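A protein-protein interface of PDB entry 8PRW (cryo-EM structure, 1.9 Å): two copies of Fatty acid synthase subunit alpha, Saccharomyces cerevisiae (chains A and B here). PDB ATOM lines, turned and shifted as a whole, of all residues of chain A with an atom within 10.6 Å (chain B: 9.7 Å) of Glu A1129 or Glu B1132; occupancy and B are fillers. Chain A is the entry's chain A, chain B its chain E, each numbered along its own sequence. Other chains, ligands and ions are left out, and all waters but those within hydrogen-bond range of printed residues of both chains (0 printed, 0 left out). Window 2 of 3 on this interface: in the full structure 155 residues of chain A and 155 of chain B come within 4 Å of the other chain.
O of Pro B1133 lies close to OE1 of Glu A1128 (3.1 Å).
O of Leu A1173 sits at hydrogen-bond distance from N of Val A1125, at 2.8 Å.
N of Leu B1131 is in hydrogen-bond range of O of Leu B1167 (2.9 Å).
N of Val B1165 sits at hydrogen-bond distance from O of Phe B1134 (2.7 Å).
Glu A1129 touches Glu B1132, and with the chains exchanged Glu A1132 touches Glu B1129.
Leu A1173 touches its own counterpart, Leu B1173.
Printed residues of chain B within 4 Å of Glu A1128: Pro B1133 and Phe B1134.
Of chain B, only Glu B1132 (3.96 Å) comes within 4 Å of Glu A1129.
No residue of chain B comes within 4 Å of Asp A1130.
Of the printed residues of chain B, Glu A1132 touches Glu B1129 (3.96 Å).
Lys A1169 touches none of the printed residues of chain B.
Printed residues of chain B within 4 Å of Ile A1175: Phe B1134, Leu B1167 and Leu B1173.
Printed residues of chain A within 4 Å of Glu B1129: Glu A1132.
Glu B1132 touches just one residue of chain A: Glu A1129.
Pro B1133 touches just one residue of chain A: Glu A1128 (3.1 Å).
Of the printed residues of chain A, Leu B1173 touches Leu A1173 (3.9 Å) and Ile A1175 (3.3 Å).
The nearest residue of chain B that does not touch Glu A1129 is Leu B1131 (6.6 Å).
The nearest residue of chain A that does not touch Glu B1132 is Glu A1128 (4.7 Å).
Glu A1128 touches Phe B1134 (OE1 to CB, 3.5 Å).
Glu B1132 touches Glu A1129.
CB of Glu B1129 touches CB of Glu A1132, 3.96 Å away.
Leu A1173 touches Leu B1173 (CD1 to CD1, 3.9 Å).
Ile A1175 touches Phe B1134 (CD1 to CE1, 3.7 Å).
CD1 of Leu B1167 touches CG2 of Ile A1175, at 3.9 Å.
Ile A1175 touches Leu B1173.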
ATOM      1  N   VAL A1125       3.124  23.313  12.962  1.00  0.00           N
ATOM      2  CA  VAL A1125       2.316  22.310  13.735  1.00  0.00           C
ATOM      3  C   VAL A1125       0.836  22.675  13.678  1.00  0.00           C
ATOM      4  O   VAL A1125       0.499  23.861  13.842  1.00  0.00           O
ATOM      5  CB  VAL A1125       2.763  22.232  15.186  1.00  0.00           C
ATOM      6  CG1 VAL A1125       4.257  21.933  15.291  1.00  0.00           C
ATOM      7  CG2 VAL A1125       2.393  23.497  15.915  1.00  0.00           C
ATOM      8  N   ILE A1126      -0.009  21.683  13.430  1.00  0.00           N
ATOM      9  CA  ILE A1126      -1.477  21.873  13.533  1.00  0.00           C
ATOM     10  C   ILE A1126      -1.834  21.827  15.021  1.00  0.00           C
ATOM     11  O   ILE A1126      -1.575  20.832  15.649  1.00  0.00           O
ATOM     12  CB  ILE A1126      -2.245  20.861  12.679  1.00  0.00           C
ATOM     13  CG1 ILE A1126      -1.716  20.795  11.243  1.00  0.00           C
ATOM     14  CG2 ILE A1126      -3.733  21.177  12.720  1.00  0.00           C
ATOM     15  CD1 ILE A1126      -1.727  22.109  10.511  1.00  0.00           C
ATOM     16  N   VAL A1127      -2.328  22.942  15.552  1.00  0.00           N
ATOM     17  CA  VAL A1127      -2.975  23.080  16.892  1.00  0.00           C
ATOM     18  C   VAL A1127      -3.973  21.914  17.060  1.00  0.00           C
ATOM     19  O   VAL A1127      -4.831  21.739  16.179  1.00  0.00           O
ATOM     20  CB  VAL A1127      -3.676  24.456  16.971  1.00  0.00           C
ATOM     21  CG1 VAL A1127      -4.551  24.617  18.191  1.00  0.00           C
ATOM     22  CG2 VAL A1127      -2.681  25.601  16.934  1.00  0.00           C
ATOM     23  N   GLU A1128      -3.832  21.084  18.090  1.00  0.00           N
ATOM     24  CA  GLU A1128      -4.786  19.962  18.346  1.00  0.00           C
ATOM     25  C   GLU A1128      -5.902  20.463  19.259  1.00  0.00           C
ATOM     26  O   GLU A1128      -7.001  19.906  19.180  1.00  0.00           O
ATOM     27  CB  GLU A1128      -4.086  18.758  18.970  1.00  0.00           C
ATOM     28  CG  GLU A1128      -3.083  18.090  18.036  1.00  0.00           C
ATOM     29  CD  GLU A1128      -1.980  17.290  18.725  1.00  0.00           C
ATOM     30  OE1 GLU A1128      -1.643  17.606  19.895  1.00  0.00           O
ATOM     31  OE2 GLU A1128      -1.448  16.351  18.090  1.00  0.00           O
ATOM     32  N   GLU A1129      -5.620  21.474  20.082  1.00  0.00           N
ATOM     33  CA  GLU A1129      -6.586  22.068  21.035  1.00  0.00           C
ATOM     34  C   GLU A1129      -6.477  23.591  21.038  1.00  0.00           C
ATOM     35  O   GLU A1129      -5.357  24.113  20.949  1.00  0.00           O
ATOM     36  CB  GLU A1129      -6.322  21.517  22.437  1.00  0.00           C
ATOM     37  CG  GLU A1129      -6.935  20.167  22.668  1.00  0.00           C
ATOM     38  CD  GLU A1129      -8.410  20.178  23.023  1.00  0.00           C
ATOM     39  OE1 GLU A1129      -9.185  21.110  22.616  1.00  0.00           O
ATOM     40  OE2 GLU A1129      -8.783  19.225  23.703  1.00  0.00           O
ATOM     41  N   ASP A1130      -7.602  24.276  21.225  1.00  0.00           N
ATOM     42  CA  ASP A1130      -7.669  25.759  21.204  1.00  0.00           C
ATOM     43  C   ASP A1130      -6.632  26.315  22.175  1.00  0.00           C
ATOM     44  O   ASP A1130      -6.422  25.717  23.240  1.00  0.00           O
ATOM     45  CB  ASP A1130      -9.083  26.283  21.480  1.00  0.00           C
ATOM     46  CG  ASP A1130     -10.122  25.706  20.527  1.00  0.00           C
ATOM     47  OD1 ASP A1130      -9.890  24.597  19.995  1.00  0.00           O
ATOM     48  OD2 ASP A1130     -11.152  26.360  20.313  1.00  0.00           O
ATOM     49  N   LEU A1131      -5.974  27.399  21.788  1.00  0.00           N
ATOM     50  CA  LEU A1131      -4.971  28.069  22.641  1.00  0.00           C
ATOM     51  C   LEU A1131      -5.711  28.968  23.615  1.00  0.00           C
ATOM     52  O   LEU A1131      -6.831  29.387  23.307  1.00  0.00           O
ATOM     53  CB  LEU A1131      -4.009  28.901  21.797  1.00  0.00           C
ATOM     54  CG  LEU A1131      -2.741  28.201  21.341  1.00  0.00           C
ATOM     55  CD1 LEU A1131      -3.077  27.058  20.408  1.00  0.00           C
ATOM     56  CD2 LEU A1131      -1.827  29.209  20.667  1.00  0.00           C
ATOM     57  N   GLU A1132      -5.060  29.269  24.730  1.00  0.00           N
ATOM     58  CA  GLU A1132      -5.473  30.355  25.639  1.00  0.00           C
ATOM     59  C   GLU A1132      -5.537  31.622  24.789  1.00  0.00           C
ATOM     60  O   GLU A1132      -4.588  31.938  24.076  1.00  0.00           O
ATOM     61  CB  GLU A1132      -4.502  30.442  26.822  1.00  0.00           C
ATOM     62  CG  GLU A1132      -4.920  31.424  27.907  1.00  0.00           C
ATOM     63  CD  GLU A1132      -6.115  31.029  28.772  1.00  0.00           C
ATOM     64  OE1 GLU A1132      -6.662  29.909  28.595  1.00  0.00           O
ATOM     65  OE2 GLU A1132      -6.505  31.852  29.630  1.00  0.00           O
ATOM     66  N   PRO A1133      -6.662  32.365  24.810  1.00  0.00           N
ATOM     67  CA  PRO A1133      -6.721  33.687  24.199  1.00  0.00           C
ATOM     68  C   PRO A1133      -5.546  34.570  24.612  1.00  0.00           C
ATOM     69  O   PRO A1133      -5.079  34.449  25.726  1.00  0.00           O
ATOM     70  CB  PRO A1133      -8.016  34.284  24.763  1.00  0.00           C
ATOM     71  CG  PRO A1133      -8.895  33.078  24.957  1.00  0.00           C
ATOM     72  CD  PRO A1133      -7.952  31.976  25.399  1.00  0.00           C
ATOM     73  N   LYS A1151     -10.339  29.267  11.729  1.00  0.00           N
ATOM     74  CA  LYS A1151      -9.478  28.647  12.775  1.00  0.00           C
ATOM     75  C   LYS A1151      -9.052  29.690  13.781  1.00  0.00           C
ATOM     76  O   LYS A1151      -8.203  29.373  14.630  1.00  0.00           O
ATOM     77  CB  LYS A1151      -8.327  27.861  12.167  1.00  0.00           C
ATOM     78  CG  LYS A1151      -8.743  26.764  11.207  1.00  0.00           C
ATOM     79  CD  LYS A1151      -9.432  25.641  11.920  1.00  0.00           C
ATOM     80  CE  LYS A1151      -9.566  24.413  11.047  1.00  0.00           C
ATOM     81  NZ  LYS A1151     -10.353  24.700   9.828  1.00  0.00           N
ATOM     82  N   LYS A1166      -8.076  34.147  19.603  1.00  0.00           N
ATOM     83  CA  LYS A1166      -8.309  32.801  20.091  1.00  0.00           C
ATOM     84  C   LYS A1166      -8.086  31.899  18.906  1.00  0.00           C
ATOM     85  O   LYS A1166      -8.944  31.836  18.067  1.00  0.00           O
ATOM     86  CB  LYS A1166      -9.706  32.625  20.706  1.00  0.00           C
ATOM     87  CG  LYS A1166      -9.971  31.189  21.150  1.00  0.00           C
ATOM     88  CD  LYS A1166     -11.196  31.005  22.019  1.00  0.00           C
ATOM     89  CE  LYS A1166     -11.497  29.543  22.307  1.00  0.00           C
ATOM     90  NZ  LYS A1166     -10.641  29.006  23.393  1.00  0.00           N
ATOM     91  N   LEU A1167      -6.909  31.260  18.882  1.00  0.00           N
ATOM     92  CA  LEU A1167      -6.542  30.270  17.861  1.00  0.00           C
ATOM     93  C   LEU A1167      -7.251  28.981  18.213  1.00  0.00           C
ATOM     94  O   LEU A1167      -7.063  28.509  19.325  1.00  0.00           O
ATOM     95  CB  LEU A1167      -5.028  30.028  17.861  1.00  0.00           C
ATOM     96  CG  LEU A1167      -4.154  30.751  16.840  1.00  0.00           C
ATOM     97  CD1 LEU A1167      -2.850  29.978  16.710  1.00  0.00           C
ATOM     98  CD2 LEU A1167      -4.786  30.868  15.458  1.00  0.00           C
ATOM     99  N   LEU A1168      -7.925  28.382  17.253  1.00  0.00           N
ATOM    100  CA  LEU A1168      -8.765  27.190  17.474  1.00  0.00           C
ATOM    101  C   LEU A1168      -8.049  25.972  16.934  1.00  0.00           C
ATOM    102  O   LEU A1168      -7.183  26.129  16.058  1.00  0.00           O
ATOM    103  CB  LEU A1168     -10.101  27.379  16.743  1.00  0.00           C
ATOM    104  CG  LEU A1168     -10.782  28.712  17.018  1.00  0.00           C
ATOM    105  CD1 LEU A1168     -12.020  28.863  16.173  1.00  0.00           C
ATOM    106  CD2 LEU A1168     -11.124  28.856  18.495  1.00  0.00           C
ATOM    107  N   LYS A1169      -8.453  24.814  17.437  1.00  0.00           N
ATOM    108  CA  LYS A1169      -8.120  23.476  16.910  1.00  0.00           C
ATOM    109  C   LYS A1169      -8.073  23.555  15.389  1.00  0.00           C
ATOM    110  O   LYS A1169      -8.984  24.138  14.807  1.00  0.00           O
ATOM    111  CB  LYS A1169      -9.157  22.457  17.409  1.00  0.00           C
ATOM    112  CG  LYS A1169      -8.996  21.038  16.883  1.00  0.00           C
ATOM    113  CD  LYS A1169      -9.833  20.005  17.639  1.00  0.00           C
ATOM    114  CE  LYS A1169      -9.427  18.562  17.388  1.00  0.00           C
ATOM    115  NZ  LYS A1169      -9.024  18.301  15.981  1.00  0.00           N
ATOM    116  N   GLY A1170      -7.037  22.969  14.787  1.00  0.00           N
ATOM    117  CA  GLY A1170      -6.867  22.908  13.323  1.00  0.00           C
ATOM    118  C   GLY A1170      -6.060  24.077  12.765  1.00  0.00           C
ATOM    119  O   GLY A1170      -5.636  23.958  11.624  1.00  0.00           O
ATOM    120  N   ALA A1171      -5.901  25.176  13.501  1.00  0.00           N
ATOM    121  CA  ALA A1171      -5.022  26.308  13.122  1.00  0.00           C
ATOM    122  C   ALA A1171      -3.546  25.863  13.032  1.00  0.00           C
ATOM    123  O   ALA A1171      -3.123  24.955  13.734  1.00  0.00           O
ATOM    124  CB  ALA A1171      -5.160  27.449  14.088  1.00  0.00           C
ATOM    125  N   THR A1172      -2.796  26.515  12.154  1.00  0.00           N
ATOM    126  CA  THR A1172      -1.354  26.285  11.885  1.00  0.00           C
ATOM    127  C   THR A1172      -0.567  27.246  12.746  1.00  0.00           C
ATOM    128  O   THR A1172      -0.892  28.443  12.754  1.00  0.00           O
ATOM    129  CB  THR A1172      -1.028  26.539  10.415  1.00  0.00           C
ATOM    130  OG1 THR A1172      -1.742  25.543   9.690  1.00  0.00           O
ATOM    131  CG2 THR A1172       0.450  26.475  10.098  1.00  0.00           C
ATOM    132  N   LEU A1173       0.414  26.730  13.462  1.00  0.00           N
ATOM    133  CA  LEU A1173       1.354  27.508  14.295  1.00  0.00           C
ATOM    134  C   LEU A1173       2.767  27.142  13.776  1.00  0.00           C
ATOM    135  O   LEU A1173       2.944  26.054  13.244  1.00  0.00           O
ATOM    136  CB  LEU A1173       1.287  27.039  15.767  1.00  0.00           C
ATOM    137  CG  LEU A1173       0.230  27.638  16.679  1.00  0.00           C
ATOM    138  CD1 LEU A1173       0.280  26.992  18.050  1.00  0.00           C
ATOM    139  CD2 LEU A1173       0.434  29.117  16.827  1.00  0.00           C
ATOM    140  N   ILE A1175       6.552  26.511  15.545  1.00  0.00           N
ATOM    141  CA  ILE A1175       7.274  26.347  16.828  1.00  0.00           C
ATOM    142  C   ILE A1175       8.746  26.307  16.537  1.00  0.00           C
ATOM    143  O   ILE A1175       9.143  25.471  15.764  1.00  0.00           O
ATOM    144  CB  ILE A1175       6.828  25.070  17.558  1.00  0.00           C
ATOM    145  CG1 ILE A1175       5.314  25.155  17.813  1.00  0.00           C
ATOM    146  CG2 ILE A1175       7.625  24.936  18.846  1.00  0.00           C
ATOM    147  CD1 ILE A1175       4.738  23.906  18.372  1.00  0.00           C
ATOM    148  N   VAL B1127       3.881  32.360  24.648  1.00  0.00           N
ATOM    149  CA  VAL B1127       2.898  31.412  25.258  1.00  0.00           C
ATOM    150  C   VAL B1127       2.568  31.920  26.678  1.00  0.00           C
ATOM    151  O   VAL B1127       3.506  32.135  27.463  1.00  0.00           O
ATOM    152  CB  VAL B1127       3.515  29.995  25.280  1.00  0.00           C
ATOM    153  CG1 VAL B1127       2.705  28.999  26.074  1.00  0.00           C
ATOM    154  CG2 VAL B1127       3.722  29.445  23.880  1.00  0.00           C
ATOM    155  N   GLU B1129       0.118  30.330  28.550  1.00  0.00           N
ATOM    156  CA  GLU B1129      -0.270  29.065  29.217  1.00  0.00           C
ATOM    157  C   GLU B1129       0.264  27.861  28.446  1.00  0.00           C
ATOM    158  O   GLU B1129       0.255  27.890  27.207  1.00  0.00           O
ATOM    159  CB  GLU B1129      -1.793  28.991  29.323  1.00  0.00           C
ATOM    160  CG  GLU B1129      -2.343  29.763  30.489  1.00  0.00           C
ATOM    161  CD  GLU B1129      -2.286  29.044  31.824  1.00  0.00           C
ATOM    162  OE1 GLU B1129      -1.352  28.214  32.088  1.00  0.00           O
ATOM    163  OE2 GLU B1129      -3.197  29.323  32.608  1.00  0.00           O
ATOM    164  N   ASP B1130       0.636  26.802  29.162  1.00  0.00           N
ATOM    165  CA  ASP B1130       1.221  25.576  28.563  1.00  0.00           C
ATOM    166  C   ASP B1130       0.298  25.076  27.456  1.00  0.00           C
ATOM    167  O   ASP B1130      -0.929  25.170  27.608  1.00  0.00           O
ATOM    168  CB  ASP B1130       1.525  24.501  29.613  1.00  0.00           C
ATOM    169  CG  ASP B1130       2.425  25.011  30.732  1.00  0.00           C
ATOM    170  OD1 ASP B1130       3.127  24.192  31.340  1.00  0.00           O
ATOM    171  OD2 ASP B1130       2.423  26.236  30.987  1.00  0.00           O
ATOM    172  N   LEU B1131       0.878  24.606  26.361  1.00  0.00           N
ATOM    173  CA  LEU B1131       0.112  24.052  25.227  1.00  0.00           C
ATOM    174  C   LEU B1131      -0.239  22.613  25.556  1.00  0.00           C
ATOM    175  O   LEU B1131       0.475  21.992  26.351  1.00  0.00           O
ATOM    176  CB  LEU B1131       0.931  24.103  23.940  1.00  0.00           C
ATOM    177  CG  LEU B1131       0.760  25.347  23.087  1.00  0.00           C
ATOM    178  CD1 LEU B1131       1.257  26.568  23.828  1.00  0.00           C
ATOM    179  CD2 LEU B1131       1.505  25.162  21.777  1.00  0.00           C
ATOM    180  N   GLU B1132      -1.288  22.114  24.919  1.00  0.00           N
ATOM    181  CA  GLU B1132      -1.594  20.672  24.870  1.00  0.00           C
ATOM    182  C   GLU B1132      -0.349  19.990  24.307  1.00  0.00           C
ATOM    183  O   GLU B1132       0.164  20.400  23.270  1.00  0.00           O
ATOM    184  CB  GLU B1132      -2.865  20.435  24.047  1.00  0.00           C
ATOM    185  CG  GLU B1132      -3.366  18.998  24.062  1.00  0.00           C
ATOM    186  CD  GLU B1132      -3.983  18.498  25.368  1.00  0.00           C
ATOM    187  OE1 GLU B1132      -4.100  19.289  26.339  1.00  0.00           O
ATOM    188  OE2 GLU B1132      -4.346  17.302  25.415  1.00  0.00           O
ATOM    189  N   PRO B1133       0.193  18.957  24.986  1.00  0.00           N
ATOM    190  CA  PRO B1133       1.242  18.128  24.411  1.00  0.00           C
ATOM    191  C   PRO B1133       0.902  17.658  22.997  1.00  0.00           C
ATOM    192  O   PRO B1133      -0.255  17.437  22.710  1.00  0.00           O
ATOM    193  CB  PRO B1133       1.287  16.910  25.342  1.00  0.00           C
ATOM    194  CG  PRO B1133       0.889  17.484  26.675  1.00  0.00           C
ATOM    195  CD  PRO B1133      -0.153  18.537  26.352  1.00  0.00           C
ATOM    196  N   PHE B1134       1.924  17.508  22.167  1.00  0.00           N
ATOM    197  CA  PHE B1134       1.812  16.914  20.820  1.00  0.00           C
ATOM    198  C   PHE B1134       2.966  15.934  20.672  1.00  0.00           C
ATOM    199  O   PHE B1134       3.915  16.025  21.419  1.00  0.00           O
ATOM    200  CB  PHE B1134       1.794  17.986  19.719  1.00  0.00           C
ATOM    201  CG  PHE B1134       3.057  18.807  19.554  1.00  0.00           C
ATOM    202  CD1 PHE B1134       3.232  19.974  20.275  1.00  0.00           C
ATOM    203  CD2 PHE B1134       4.075  18.394  18.710  1.00  0.00           C
ATOM    204  CE1 PHE B1134       4.389  20.727  20.137  1.00  0.00           C
ATOM    205  CE2 PHE B1134       5.242  19.132  18.588  1.00  0.00           C
ATOM    206  CZ  PHE B1134       5.389  20.300  19.299  1.00  0.00           C
ATOM    207  N   GLU B1135       2.829  15.020  19.740  1.00  0.00           N
ATOM    208  CA  GLU B1135       3.755  13.894  19.526  1.00  0.00           C
ATOM    209  C   GLU B1135       4.746  14.354  18.468  1.00  0.00           C
ATOM    210  O   GLU B1135       4.334  15.062  17.524  1.00  0.00           O
ATOM    211  CB  GLU B1135       2.981  12.668  19.039  1.00  0.00           C
ATOM    212  CG  GLU B1135       3.337  11.380  19.764  1.00  0.00           C
ATOM    213  CD  GLU B1135       2.503  10.185  19.300  1.00  0.00           C
ATOM    214  OE1 GLU B1135       2.866   9.580  18.260  1.00  0.00           O
ATOM    215  OE2 GLU B1135       1.480   9.875  19.966  1.00  0.00           O
ATOM    216  N   VAL B1152      10.251  23.962  27.570  1.00  0.00           N
ATOM    217  CA  VAL B1152       9.621  22.794  26.934  1.00  0.00           C
ATOM    218  C   VAL B1152      10.001  21.558  27.732  1.00  0.00           C
ATOM    219  O   VAL B1152      11.116  21.495  28.255  1.00  0.00           O
ATOM    220  CB  VAL B1152       9.984  22.623  25.431  1.00  0.00           C
ATOM    221  CG1 VAL B1152      11.397  22.155  25.215  1.00  0.00           C
ATOM    222  CG2 VAL B1152       9.072  21.678  24.704  1.00  0.00           C
ATOM    223  N   ASP B1153       9.089  20.591  27.728  1.00  0.00           N
ATOM    224  CA  ASP B1153       9.322  19.263  28.315  1.00  0.00           C
ATOM    225  C   ASP B1153       9.016  18.262  27.260  1.00  0.00           C
ATOM    226  O   ASP B1153       7.982  18.375  26.587  1.00  0.00           O
ATOM    227  CB  ASP B1153       8.419  18.935  29.514  1.00  0.00           C
ATOM    228  CG  ASP B1153       8.790  19.744  30.742  1.00  0.00           C
ATOM    229  OD1 ASP B1153       9.996  19.821  31.049  1.00  0.00           O
ATOM    230  OD2 ASP B1153       7.871  20.322  31.364  1.00  0.00           O
ATOM    231  N   SER B1164       6.563  13.035  23.588  1.00  0.00           N
ATOM    232  CA  SER B1164       5.541  14.059  23.819  1.00  0.00           C
ATOM    233  C   SER B1164       6.329  15.346  23.865  1.00  0.00           C
ATOM    234  O   SER B1164       7.392  15.356  24.469  1.00  0.00           O
ATOM    235  CB  SER B1164       4.738  13.847  25.089  1.00  0.00           C
ATOM    236  OG  SER B1164       5.496  14.250  26.230  1.00  0.00           O
ATOM    237  N   VAL B1165       5.771  16.406  23.314  1.00  0.00           N
ATOM    238  CA  VAL B1165       6.421  17.721  23.405  1.00  0.00           C
ATOM    239  C   VAL B1165       5.427  18.628  24.065  1.00  0.00           C
ATOM    240  O   VAL B1165       4.325  18.781  23.543  1.00  0.00           O
ATOM    241  CB  VAL B1165       6.850  18.235  22.009  1.00  0.00           C
ATOM    242  CG1 VAL B1165       7.459  19.614  22.115  1.00  0.00           C
ATOM    243  CG2 VAL B1165       7.791  17.267  21.342  1.00  0.00           C
ATOM    244  N   LYS B1166       5.862  19.286  25.101  1.00  0.00           N
ATOM    245  CA  LYS B1166       4.986  20.084  25.939  1.00  0.00           C
ATOM    246  C   LYS B1166       5.655  21.427  26.058  1.00  0.00           C
ATOM    247  O   LYS B1166       6.599  21.531  26.795  1.00  0.00           O
ATOM    248  CB  LYS B1166       4.723  19.436  27.308  1.00  0.00           C
ATOM    249  CG  LYS B1166       3.862  20.314  28.212  1.00  0.00           C
ATOM    250  CD  LYS B1166       3.325  19.627  29.448  1.00  0.00           C
ATOM    251  CE  LYS B1166       2.603  20.580  30.385  1.00  0.00           C
ATOM    252  NZ  LYS B1166       1.217  20.854  29.931  1.00  0.00           N
ATOM    253  N   LEU B1167       5.144  22.395  25.287  1.00  0.00           N
ATOM    254  CA  LEU B1167       5.596  23.791  25.326  1.00  0.00           C
ATOM    255  C   LEU B1167       4.983  24.425  26.556  1.00  0.00           C
ATOM    256  O   LEU B1167       3.766  24.388  26.674  1.00  0.00           O
ATOM    257  CB  LEU B1167       5.125  24.549  24.081  1.00  0.00           C
ATOM    258  CG  LEU B1167       6.084  24.738  22.910  1.00  0.00           C
ATOM    259  CD1 LEU B1167       5.585  25.912  22.079  1.00  0.00           C
ATOM    260  CD2 LEU B1167       7.522  25.020  23.328  1.00  0.00           C
ATOM    261  N   LEU B1168       5.789  25.090  27.358  1.00  0.00           N
ATOM    262  CA  LEU B1168       5.363  25.654  28.652  1.00  0.00           C
ATOM    263  C   LEU B1168       5.213  27.153  28.515  1.00  0.00           C
ATOM    264  O   LEU B1168       5.836  27.735  27.611  1.00  0.00           O
ATOM    265  CB  LEU B1168       6.422  25.329  29.711  1.00  0.00           C
ATOM    266  CG  LEU B1168       6.842  23.867  29.750  1.00  0.00           C
ATOM    267  CD1 LEU B1168       7.967  23.659  30.731  1.00  0.00           C
ATOM    268  CD2 LEU B1168       5.663  22.968  30.093  1.00  0.00           C
ATOM    269  N   LYS B1169       4.436  27.726  29.423  1.00  0.00           N
ATOM    270  CA  LYS B1169       4.328  29.175  29.682  1.00  0.00           C
ATOM    271  C   LYS B1169       5.704  29.802  29.501  1.00  0.00           C
ATOM    272  O   LYS B1169       6.670  29.247  30.017  1.00  0.00           O
ATOM    273  CB  LYS B1169       3.765  29.401  31.095  1.00  0.00           C
ATOM    274  CG  LYS B1169       3.668  30.851  31.543  1.00  0.00           C
ATOM    275  CD  LYS B1169       2.821  31.050  32.801  1.00  0.00           C
ATOM    276  CE  LYS B1169       2.408  32.491  33.059  1.00  0.00           C
ATOM    277  NZ  LYS B1169       3.468  33.476  32.717  1.00  0.00           N
ATOM    278  N   LEU B1173       6.458  31.207  20.376  1.00  0.00           N
ATOM    279  CA  LEU B1173       5.765  30.551  19.247  1.00  0.00           C
ATOM    280  C   LEU B1173       5.739  31.603  18.111  1.00  0.00           C
ATOM    281  O   LEU B1173       5.765  32.793  18.398  1.00  0.00           O
ATOM    282  CB  LEU B1173       4.292  30.258  19.616  1.00  0.00           C
ATOM    283  CG  LEU B1173       3.964  28.973  20.359  1.00  0.00           C
ATOM    284  CD1 LEU B1173       2.487  28.914  20.695  1.00  0.00           C
ATOM    285  CD2 LEU B1173       4.328  27.776  19.532  1.00  0.00           C
